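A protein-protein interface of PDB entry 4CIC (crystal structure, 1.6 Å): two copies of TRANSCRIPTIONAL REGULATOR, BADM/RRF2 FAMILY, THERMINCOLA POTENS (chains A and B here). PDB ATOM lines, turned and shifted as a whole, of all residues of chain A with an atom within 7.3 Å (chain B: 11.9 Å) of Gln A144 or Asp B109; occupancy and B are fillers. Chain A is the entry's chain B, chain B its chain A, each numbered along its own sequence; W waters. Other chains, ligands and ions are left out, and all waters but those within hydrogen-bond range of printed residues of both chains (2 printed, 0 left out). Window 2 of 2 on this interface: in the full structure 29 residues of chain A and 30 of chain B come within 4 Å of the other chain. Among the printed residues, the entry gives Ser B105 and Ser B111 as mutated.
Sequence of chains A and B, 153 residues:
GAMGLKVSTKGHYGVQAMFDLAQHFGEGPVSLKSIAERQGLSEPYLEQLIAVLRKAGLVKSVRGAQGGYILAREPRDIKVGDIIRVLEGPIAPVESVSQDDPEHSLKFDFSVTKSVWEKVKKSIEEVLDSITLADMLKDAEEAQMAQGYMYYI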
ATOM      1  N   GLN A  16      11.837  30.580  29.700  1.00  0.00           N
ATOM      2  CA  GLN A  16      10.661  29.720  29.878  1.00  0.00           C
ATOM      3  C   GLN A  16       9.451  30.289  29.163  1.00  0.00           C
ATOM      4  O   GLN A  16       8.719  29.556  28.492  1.00  0.00           O
ATOM      5  CB  GLN A  16      10.306  29.546  31.352  1.00  0.00           C
ATOM      6  CG  GLN A  16      11.007  28.390  32.029  1.00  0.00           C
ATOM      7  CD  GLN A  16      10.516  28.206  33.454  1.00  0.00           C
ATOM      8  OE1 GLN A  16      10.955  28.907  34.364  1.00  0.00           O
ATOM      9  NE2 GLN A  16       9.600  27.276  33.649  1.00  0.00           N
ATOM     10  N   PHE A  19       9.854  30.160  25.387  1.00  0.00           N
ATOM     11  CA  PHE A  19       9.714  28.796  24.894  1.00  0.00           C
ATOM     12  C   PHE A  19       8.246  28.362  24.897  1.00  0.00           C
ATOM     13  O   PHE A  19       7.794  27.678  23.975  1.00  0.00           O
ATOM     14  CB  PHE A  19      10.561  27.804  25.686  1.00  0.00           C
ATOM     15  CG  PHE A  19      10.481  26.406  25.155  1.00  0.00           C
ATOM     16  CD1 PHE A  19      10.955  26.100  23.880  1.00  0.00           C
ATOM     17  CD2 PHE A  19       9.890  25.407  25.908  1.00  0.00           C
ATOM     18  CE1 PHE A  19      10.843  24.784  23.374  1.00  0.00           C
ATOM     19  CE2 PHE A  19       9.771  24.114  25.407  1.00  0.00           C
ATOM     20  CZ  PHE A  19      10.267  23.804  24.144  1.00  0.00           C
ATOM     21  N   GLN A  23       6.106  26.938  21.736  1.00  0.00           N
ATOM     22  CA  GLN A  23       5.333  25.695  21.736  1.00  0.00           C
ATOM     23  C   GLN A  23       3.921  25.942  21.253  1.00  0.00           C
ATOM     24  O   GLN A  23       3.241  25.014  20.825  1.00  0.00           O
ATOM     25  CB  GLN A  23       5.252  25.096  23.133  1.00  0.00           C
ATOM     26  CG  GLN A  23       6.598  24.522  23.578  1.00  0.00           C
ATOM     27  CD  GLN A  23       6.511  23.845  24.936  1.00  0.00           C
ATOM     28  OE1 GLN A  23       6.404  24.508  25.971  1.00  0.00           O
ATOM     29  NE2 GLN A  23       6.571  22.522  24.939  1.00  0.00           N
ATOM     30  N   ARG A  38       1.137  27.157  33.063  1.00  0.00           N
ATOM     31  CA  ARG A  38       1.881  26.016  32.547  1.00  0.00           C
ATOM     32  C   ARG A  38       3.323  26.013  33.038  1.00  0.00           C
ATOM     33  O   ARG A  38       3.923  24.959  33.211  1.00  0.00           O
ATOM     34  CB  ARG A  38       1.878  26.014  31.019  1.00  0.00           C
ATOM     35  CG  ARG A  38       0.557  25.610  30.391  1.00  0.00           C
ATOM     36  CD  ARG A  38       0.698  25.542  28.876  1.00  0.00           C
ATOM     37  NE  ARG A  38       0.928  26.858  28.282  1.00  0.00           N
ATOM     38  CZ  ARG A  38      -0.037  27.643  27.809  1.00  0.00           C
ATOM     39  NH1 ARG A  38      -1.312  27.248  27.862  1.00  0.00           N
ATOM     40  NH2 ARG A  38       0.266  28.824  27.277  1.00  0.00           N
ATOM     41  N   GLN A  39       3.877  27.198  33.248  1.00  0.00           N
ATOM     42  CA  GLN A  39       5.300  27.321  33.560  1.00  0.00           C
ATOM     43  C   GLN A  39       5.591  27.560  35.034  1.00  0.00           C
ATOM     44  O   GLN A  39       6.754  27.619  35.443  1.00  0.00           O
ATOM     45  CB  GLN A  39       5.931  28.426  32.711  1.00  0.00           C
ATOM     46  CG  GLN A  39       5.804  28.194  31.213  1.00  0.00           C
ATOM     47  CD  GLN A  39       6.410  26.880  30.769  1.00  0.00           C
ATOM     48  OE1 GLN A  39       7.416  26.418  31.324  1.00  0.00           O
ATOM     49  NE2 GLN A  39       5.807  26.269  29.764  1.00  0.00           N
ATOM     50  N   MET A 136      15.146  24.237  20.491  1.00  0.00           N
ATOM     51  CA  MET A 136      14.524  23.822  21.748  1.00  0.00           C
ATOM     52  C   MET A 136      13.226  23.044  21.481  1.00  0.00           C
ATOM     53  O   MET A 136      12.932  22.043  22.132  1.00  0.00           O
ATOM     54  CB  MET A 136      14.276  25.040  22.644  1.00  0.00           C
ATOM     55  CG  MET A 136      15.606  25.685  23.175  1.00  0.00           C
ATOM     56  SD  MET A 136      15.267  27.171  24.106  1.00  0.00           S
ATOM     57  CE  MET A 136      14.550  26.514  25.599  1.00  0.00           C
ATOM     58  N   LYS A 138      12.590  21.176  18.831  1.00  0.00           N
ATOM     59  CA  LYS A 138      13.028  19.856  18.390  1.00  0.00           C
ATOM     60  C   LYS A 138      13.499  18.981  19.550  1.00  0.00           C
ATOM     61  O   LYS A 138      13.119  17.815  19.645  1.00  0.00           O
ATOM     62  CB  LYS A 138      14.133  19.972  17.343  1.00  0.00           C
ATOM     63  CG  LYS A 138      13.664  20.567  16.026  1.00  0.00           C
ATOM     64  CD  LYS A 138      14.851  20.847  15.123  1.00  0.00           C
ATOM     65  CE  LYS A 138      14.429  21.549  13.850  1.00  0.00           C
ATOM     66  NZ  LYS A 138      15.598  21.813  12.964  1.00  0.00           N
ATOM     67  N   ASP A 139      14.334  19.540  20.422  1.00  0.00           N
ATOM     68  CA  ASP A 139      14.798  18.804  21.592  1.00  0.00           C
ATOM     69  C   ASP A 139      13.649  18.376  22.503  1.00  0.00           C
ATOM     70  O   ASP A 139      13.650  17.258  23.026  1.00  0.00           O
ATOM     71  CB  ASP A 139      15.793  19.639  22.379  1.00  0.00           C
ATOM     72  CG  ASP A 139      17.159  19.685  21.721  1.00  0.00           C
ATOM     73  OD1 ASP A 139      17.338  19.038  20.664  1.00  0.00           O
ATOM     74  OD2 ASP A 139      18.059  20.354  22.272  1.00  0.00           O
ATOM     75  N   ALA A 140      12.684  19.276  22.691  1.00  0.00           N
ATOM     76  CA  ALA A 140      11.525  19.023  23.540  1.00  0.00           C
ATOM     77  C   ALA A 140      10.770  17.809  23.046  1.00  0.00           C
ATOM     78  O   ALA A 140      10.412  16.933  23.831  1.00  0.00           O
ATOM     79  CB  ALA A 140      10.599  20.233  23.555  1.00  0.00           C
ATOM     80  N   GLU A 141      10.526  17.768  21.742  1.00  0.00           N
ATOM     81  CA  GLU A 141       9.870  16.619  21.133  1.00  0.00           C
ATOM     82  C   GLU A 141      10.643  15.334  21.439  1.00  0.00           C
ATOM     83  O   GLU A 141      10.109  14.425  22.067  1.00  0.00           O
ATOM     84  CB  GLU A 141       9.714  16.810  19.623  1.00  0.00           C
ATOM     85  CG  GLU A 141       9.025  15.641  18.938  1.00  0.00           C
ATOM     86  CD  GLU A 141       8.793  15.874  17.459  1.00  0.00           C
ATOM     87  OE1 GLU A 141       9.526  16.691  16.864  1.00  0.00           O
ATOM     88  OE2 GLU A 141       7.875  15.240  16.894  1.00  0.00           O
ATOM     89  N   GLU A 142      11.907  15.290  21.029  1.00  0.00           N
ATOM     90  CA  GLU A 142      12.755  14.103  21.191  1.00  0.00           C
ATOM     91  C   GLU A 142      12.853  13.570  22.619  1.00  0.00           C
ATOM     92  O   GLU A 142      12.847  12.357  22.839  1.00  0.00           O
ATOM     93  CB  GLU A 142      14.168  14.384  20.673  1.00  0.00           C
ATOM     94  CG  GLU A 142      14.618  13.468  19.554  1.00  0.00           C
ATOM     95  CD  GLU A 142      14.319  14.047  18.185  1.00  0.00           C
ATOM     96  OE1 GLU A 142      14.457  15.281  18.024  1.00  0.00           O
ATOM     97  OE2 GLU A 142      13.950  13.277  17.270  1.00  0.00           O
ATOM     98  N   ALA A 143      12.953  14.474  23.587  1.00  0.00           N
ATOM     99  CA  ALA A 143      13.269  14.077  24.960  1.00  0.00           C
ATOM    100  C   ALA A 143      12.029  13.721  25.775  1.00  0.00           C
ATOM    101  O   ALA A 143      12.127  12.987  26.763  1.00  0.00           O
ATOM    102  CB  ALA A 143      14.083  15.159  25.661  1.00  0.00           C
ATOM    103  N   GLN A 144      10.874  14.237  25.360  1.00  0.00           N
ATOM    104  CA  GLN A 144       9.618  13.972  26.051  1.00  0.00           C
ATOM    105  C   GLN A 144       8.697  13.205  25.127  1.00  0.00           C
ATOM    106  O   GLN A 144       7.570  13.624  24.850  1.00  0.00           O
ATOM    107  CB  GLN A 144       8.948  15.275  26.505  1.00  0.00           C
ATOM    108  CG  GLN A 144       9.617  15.939  27.709  1.00  0.00           C
ATOM    109  CD  GLN A 144       9.179  17.384  27.916  1.00  0.00           C
ATOM    110  OE1 GLN A 144       9.346  18.225  27.031  1.00  0.00           O
ATOM    111  NE2 GLN A 144       8.623  17.678  29.091  1.00  0.00           N
ATOM    112  N   MET A 145       9.188  12.077  24.638  1.00  0.00           N
ATOM    113  CA  MET A 145       8.413  11.275  23.711  1.00  0.00           C
ATOM    114  C   MET A 145       7.972   9.975  24.373  1.00  0.00           C
ATOM    115  O   MET A 145       8.269   9.714  25.540  1.00  0.00           O
ATOM    116  CB  MET A 145       9.225  10.998  22.441  1.00  0.00           C
ATOM    117  CG  MET A 145       8.771  11.826  21.246  1.00  0.00           C
ATOM    118  SD  MET A 145      10.051  12.131  20.005  1.00  0.00           S
ATOM    119  CE  MET A 145      10.535  10.470  19.551  1.00  0.00           C
ATOM    120  N   ALA A 146       7.227   9.175  23.633  1.00  0.00           N
ATOM    121  CA  ALA A 146       6.929   7.834  24.078  1.00  0.00           C
ATOM    122  C   ALA A 146       6.921   6.957  22.843  1.00  0.00           C
ATOM    123  O   ALA A 146       6.454   7.376  21.785  1.00  0.00           O
ATOM    124  CB  ALA A 146       5.602   7.790  24.807  1.00  0.00           C
ATOM    125  N   SER B 105       3.471  14.236  45.906  1.00  0.00           N
ATOM    126  CA  SER B 105       3.784  15.634  45.630  1.00  0.00           C
ATOM    127  C   SER B 105       4.908  15.767  44.602  1.00  0.00           C
ATOM    128  O   SER B 105       5.036  16.799  43.945  1.00  0.00           O
ATOM    129  CB  SER B 105       4.151  16.370  46.923  1.00  0.00           C
ATOM    130  OG  SER B 105       5.177  15.692  47.626  1.00  0.00           O
ATOM    131  N   LEU B 106       5.716  14.718  44.465  1.00  0.00           N
ATOM    132  CA  LEU B 106       6.830  14.722  43.519  1.00  0.00           C
ATOM    133  C   LEU B 106       6.408  14.260  42.136  1.00  0.00           C
ATOM    134  O   LEU B 106       5.517  13.430  41.995  1.00  0.00           O
ATOM    135  CB  LEU B 106       7.960  13.817  44.005  1.00  0.00           C
ATOM    136  CG  LEU B 106       8.934  14.386  45.030  1.00  0.00           C
ATOM    137  CD1 LEU B 106      10.038  13.386  45.271  1.00  0.00           C
ATOM    138  CD2 LEU B 106       9.508  15.712  44.555  1.00  0.00           C
ATOM    139  N   LYS B 107       7.076  14.789  41.117  1.00  0.00           N
ATOM    140  CA  LYS B 107       6.857  14.331  39.752  1.00  0.00           C
ATOM    141  C   LYS B 107       7.991  14.801  38.868  1.00  0.00           C
ATOM    142  O   LYS B 107       8.597  15.842  39.119  1.00  0.00           O
ATOM    143  CB  LYS B 107       5.525  14.842  39.203  1.00  0.00           C
ATOM    144  CG  LYS B 107       5.497  16.335  38.926  1.00  0.00           C
ATOM    145  CD  LYS B 107       4.135  16.786  38.422  1.00  0.00           C
ATOM    146  CE  LYS B 107       4.080  18.300  38.282  1.00  0.00           C
ATOM    147  NZ  LYS B 107       2.714  18.779  37.925  1.00  0.00           N
ATOM    148  N   PHE B 108       8.294  14.024  37.838  1.00  0.00           N
ATOM    149  CA  PHE B 108       9.295  14.433  36.882  1.00  0.00           C
ATOM    150  C   PHE B 108       8.657  15.060  35.648  1.00  0.00           C
ATOM    151  O   PHE B 108       7.738  14.488  35.057  1.00  0.00           O
ATOM    152  CB  PHE B 108      10.183  13.259  36.477  1.00  0.00           C
ATOM    153  CG  PHE B 108      11.164  13.601  35.403  1.00  0.00           C
ATOM    154  CD1 PHE B 108      12.288  14.348  35.693  1.00  0.00           C
ATOM    155  CD2 PHE B 108      10.940  13.222  34.091  1.00  0.00           C
ATOM    156  CE1 PHE B 108      13.187  14.685  34.702  1.00  0.00           C
ATOM    157  CE2 PHE B 108      11.844  13.553  33.095  1.00  0.00           C
ATOM    158  CZ  PHE B 108      12.974  14.278  33.408  1.00  0.00           C
ATOM    159  N   ASP B 109       9.153  16.239  35.287  1.00  0.00           N
ATOM    160  CA  ASP B 109       8.788  16.931  34.066  1.00  0.00           C
ATOM    161  C   ASP B 109      10.057  17.538  33.485  1.00  0.00           C
ATOM    162  O   ASP B 109      10.606  18.486  34.049  1.00  0.00           O
ATOM    163  CB  ASP B 109       7.769  18.032  34.364  1.00  0.00           C
ATOM    164  CG  ASP B 109       7.697  19.077  33.264  1.00  0.00           C
ATOM    165  OD1 ASP B 109       7.161  18.767  32.182  1.00  0.00           O
ATOM    166  OD2 ASP B 109       8.176  20.214  33.483  1.00  0.00           O
ATOM    167  N   PHE B 110      10.529  16.988  32.371  1.00  0.00           N
ATOM    168  CA  PHE B 110      11.757  17.491  31.740  1.00  0.00           C
ATOM    169  C   PHE B 110      11.601  18.936  31.281  1.00  0.00           C
ATOM    170  O   PHE B 110      10.581  19.300  30.670  1.00  0.00           O
ATOM    171  CB  PHE B 110      12.172  16.594  30.573  1.00  0.00           C
ATOM    172  CG  PHE B 110      13.353  17.108  29.789  1.00  0.00           C
ATOM    173  CD1 PHE B 110      14.632  17.080  30.331  1.00  0.00           C
ATOM    174  CD2 PHE B 110      13.190  17.594  28.503  1.00  0.00           C
ATOM    175  CE1 PHE B 110      15.726  17.539  29.600  1.00  0.00           C
ATOM    176  CE2 PHE B 110      14.277  18.050  27.773  1.00  0.00           C
ATOM    177  CZ  PHE B 110      15.545  18.026  28.321  1.00  0.00           C
ATOM    178  N   SER B 111      12.614  19.749  31.594  1.00  0.00           N
ATOM    179  CA  SER B 111      12.660  21.152  31.217  1.00  0.00           C
ATOM    180  C   SER B 111      13.723  21.356  30.164  1.00  0.00           C
ATOM    181  O   SER B 111      14.923  21.235  30.456  1.00  0.00           O
ATOM    182  CB  SER B 111      13.008  22.029  32.428  1.00  0.00           C
ATOM    183  OG  SER B 111      13.205  23.377  32.032  1.00  0.00           O
ATOM    184  N   VAL B 112      13.324  21.662  28.935  1.00  0.00           N
ATOM    185  CA  VAL B 112      14.318  21.966  27.910  1.00  0.00           C
ATOM    186  C   VAL B 112      15.081  23.238  28.268  1.00  0.00           C
ATOM    187  O   VAL B 112      16.258  23.365  27.946  1.00  0.00           O
ATOM    188  CB  VAL B 112      13.685  22.105  26.504  1.00  0.00           C
ATOM    189  CG1 VAL B 112      12.813  23.324  26.446  1.00  0.00           C
ATOM    190  CG2 VAL B 112      14.776  22.180  25.443  1.00  0.00           C
ATOM    191  N   THR B 113      14.422  24.185  28.948  1.00  0.00           N
ATOM    192  CA  THR B 113      15.102  25.418  29.359  1.00  0.00           C
ATOM    193  C   THR B 113      16.252  25.103  30.316  1.00  0.00           C
ATOM    194  O   THR B 113      17.362  25.625  30.158  1.00  0.00           O
ATOM    195  CB  THR B 113      14.149  26.439  30.030  1.00  0.00           C
ATOM    196  OG1 THR B 113      13.128  26.821  29.103  1.00  0.00           O
ATOM    197  CG2 THR B 113      14.908  27.701  30.484  1.00  0.00           C
ATOM    198  N   LYS B 114      16.002  24.243  31.300  1.00  0.00           N
ATOM    199  CA  LYS B 114      17.096  23.865  32.204  1.00  0.00           C
ATOM    200  C   LYS B 114      18.227  23.183  31.448  1.00  0.00           C
ATOM    201  O   LYS B 114      19.398  23.299  31.842  1.00  0.00           O
ATOM    202  CB  LYS B 114      16.630  22.931  33.312  1.00  0.00           C
ATOM    203  CG  LYS B 114      15.737  23.571  34.350  1.00  0.00           C
ATOM    204  CD  LYS B 114      15.460  22.560  35.445  1.00  0.00           C
ATOM    205  CE  LYS B 114      14.427  23.045  36.412  1.00  0.00           C
ATOM    206  NZ  LYS B 114      14.148  22.001  37.440  1.00  0.00           N
ATOM    207  N   SER B 115      17.891  22.457  30.382  1.00  0.00           N
ATOM    208  CA  SER B 115      18.938  21.750  29.644  1.00  0.00           C
ATOM    209  C   SER B 115      19.836  22.756  28.942  1.00  0.00           C
ATOM    210  O   SER B 115      21.036  22.503  28.752  1.00  0.00           O
ATOM    211  CB  SER B 115      18.355  20.736  28.653  1.00  0.00           C
ATOM    212  OG  SER B 115      17.830  21.376  27.500  1.00  0.00           O
ATOM    213  N   VAL B 116      19.271  23.905  28.577  1.00  0.00           N
ATOM    214  CA  VAL B 116      20.089  24.965  27.984  1.00  0.00           C
ATOM    215  C   VAL B 116      21.098  25.466  29.010  1.00  0.00           C
ATOM    216  O   VAL B 116      22.287  25.635  28.686  1.00  0.00           O
ATOM    217  CB  VAL B 116      19.252  26.148  27.477  1.00  0.00           C
ATOM    218  CG1 VAL B 116      20.147  27.258  26.966  1.00  0.00           C
ATOM    219  CG2 VAL B 116      18.316  25.694  26.350  1.00  0.00           C
HETATM  220  O   HOH W   1       8.574  15.121  30.819  1.00  0.00           O
HETATM  221  O   HOH W   2      17.898  19.455  25.379  1.00  0.00           O
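The backbone NH (N) of Thr B113 sits close to the side-chain hydroxyl (OG) of Ser B111 (3.4 Å). The side-chain hydroxyl (OG) of Ser B115 is in hydrogen-bond range of the backbone carbonyl oxygen (O) of Val B112, 2.6 Å away. The side-chain amide oxygen (OE1) of Gln A39 is in hydrogen-bond range of the side-chain amide nitrogen (NE2) of Gln A16.
No position is printed for both chains. Of the 8 pairs that touch across the chains among the printed residues, none has its exchanged pair printed and touching as well.
Of the printed residues of chain B, Gln A16 touches Thr B113. Of the printed residues of chain B, Met A136 touches Val B112, Thr B113 and Val B116. Gln A144 touches just these residues of chain B: Asp B109 and Phe B110. Met A145 touches none of the printed residues of chain B. No residue of chain B comes within 4 Å of Ala A146. Ser B105 touches none of the printed residues of chain A. Of chain A, only Gln A144 (3.6 Å) comes within 4 Å of Asp B109. Printed residues of chain A within 4 Å of Phe B110: Ala A143 and Gln A144. Of the printed residues of chain A, Val B112 touches Phe A19 and Met A136. Printed residues of chain A within 4 Å of Thr B113: Gln A16 (3.9 Å) and Met A136 (3.8 Å). Ser B115 touches none of the printed residues of chain A. The nearest residue of chain A that does not touch Asp B109 is Arg A38 (6.4 Å).
Of the 12 printed residues of chain B, 5 touch a printed residue of chain A. Hydrophobic or aromatic side chains of chain B that line the printed part of chain A: Phe B110, Val B112 and Val B116. Among the printed residues, no Asp or Glu carboxylate lies within 4 Å of a Lys or Arg side-chain nitrogen of the other chain.
The side-chain amide nitrogen (NE2) of Gln A144 sits at hydrogen-bond distance from the backbone carbonyl oxygen (O) of Phe B110, 3.0 Å away.
Water W2 lies within hydrogen-bond range of OG of Ser B115 (2.9 Å) and OD2 of Asp A139 (3.2 Å). Water W1 bridges the side-chain amide nitrogen (NE2) of Gln A144 (3.1 Å) and the backbone NH (N) of Phe B110 (3.1 Å).
Among the printed residues, merely in contact across the chains: Gln A16 with Thr B113, Phe A19 with Val B112, Met A136 with Val B112, Met A136 with Thr B113, Met A136 with Val B116, Ala A143 with Phe B110 and Gln A144 with Asp B109.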
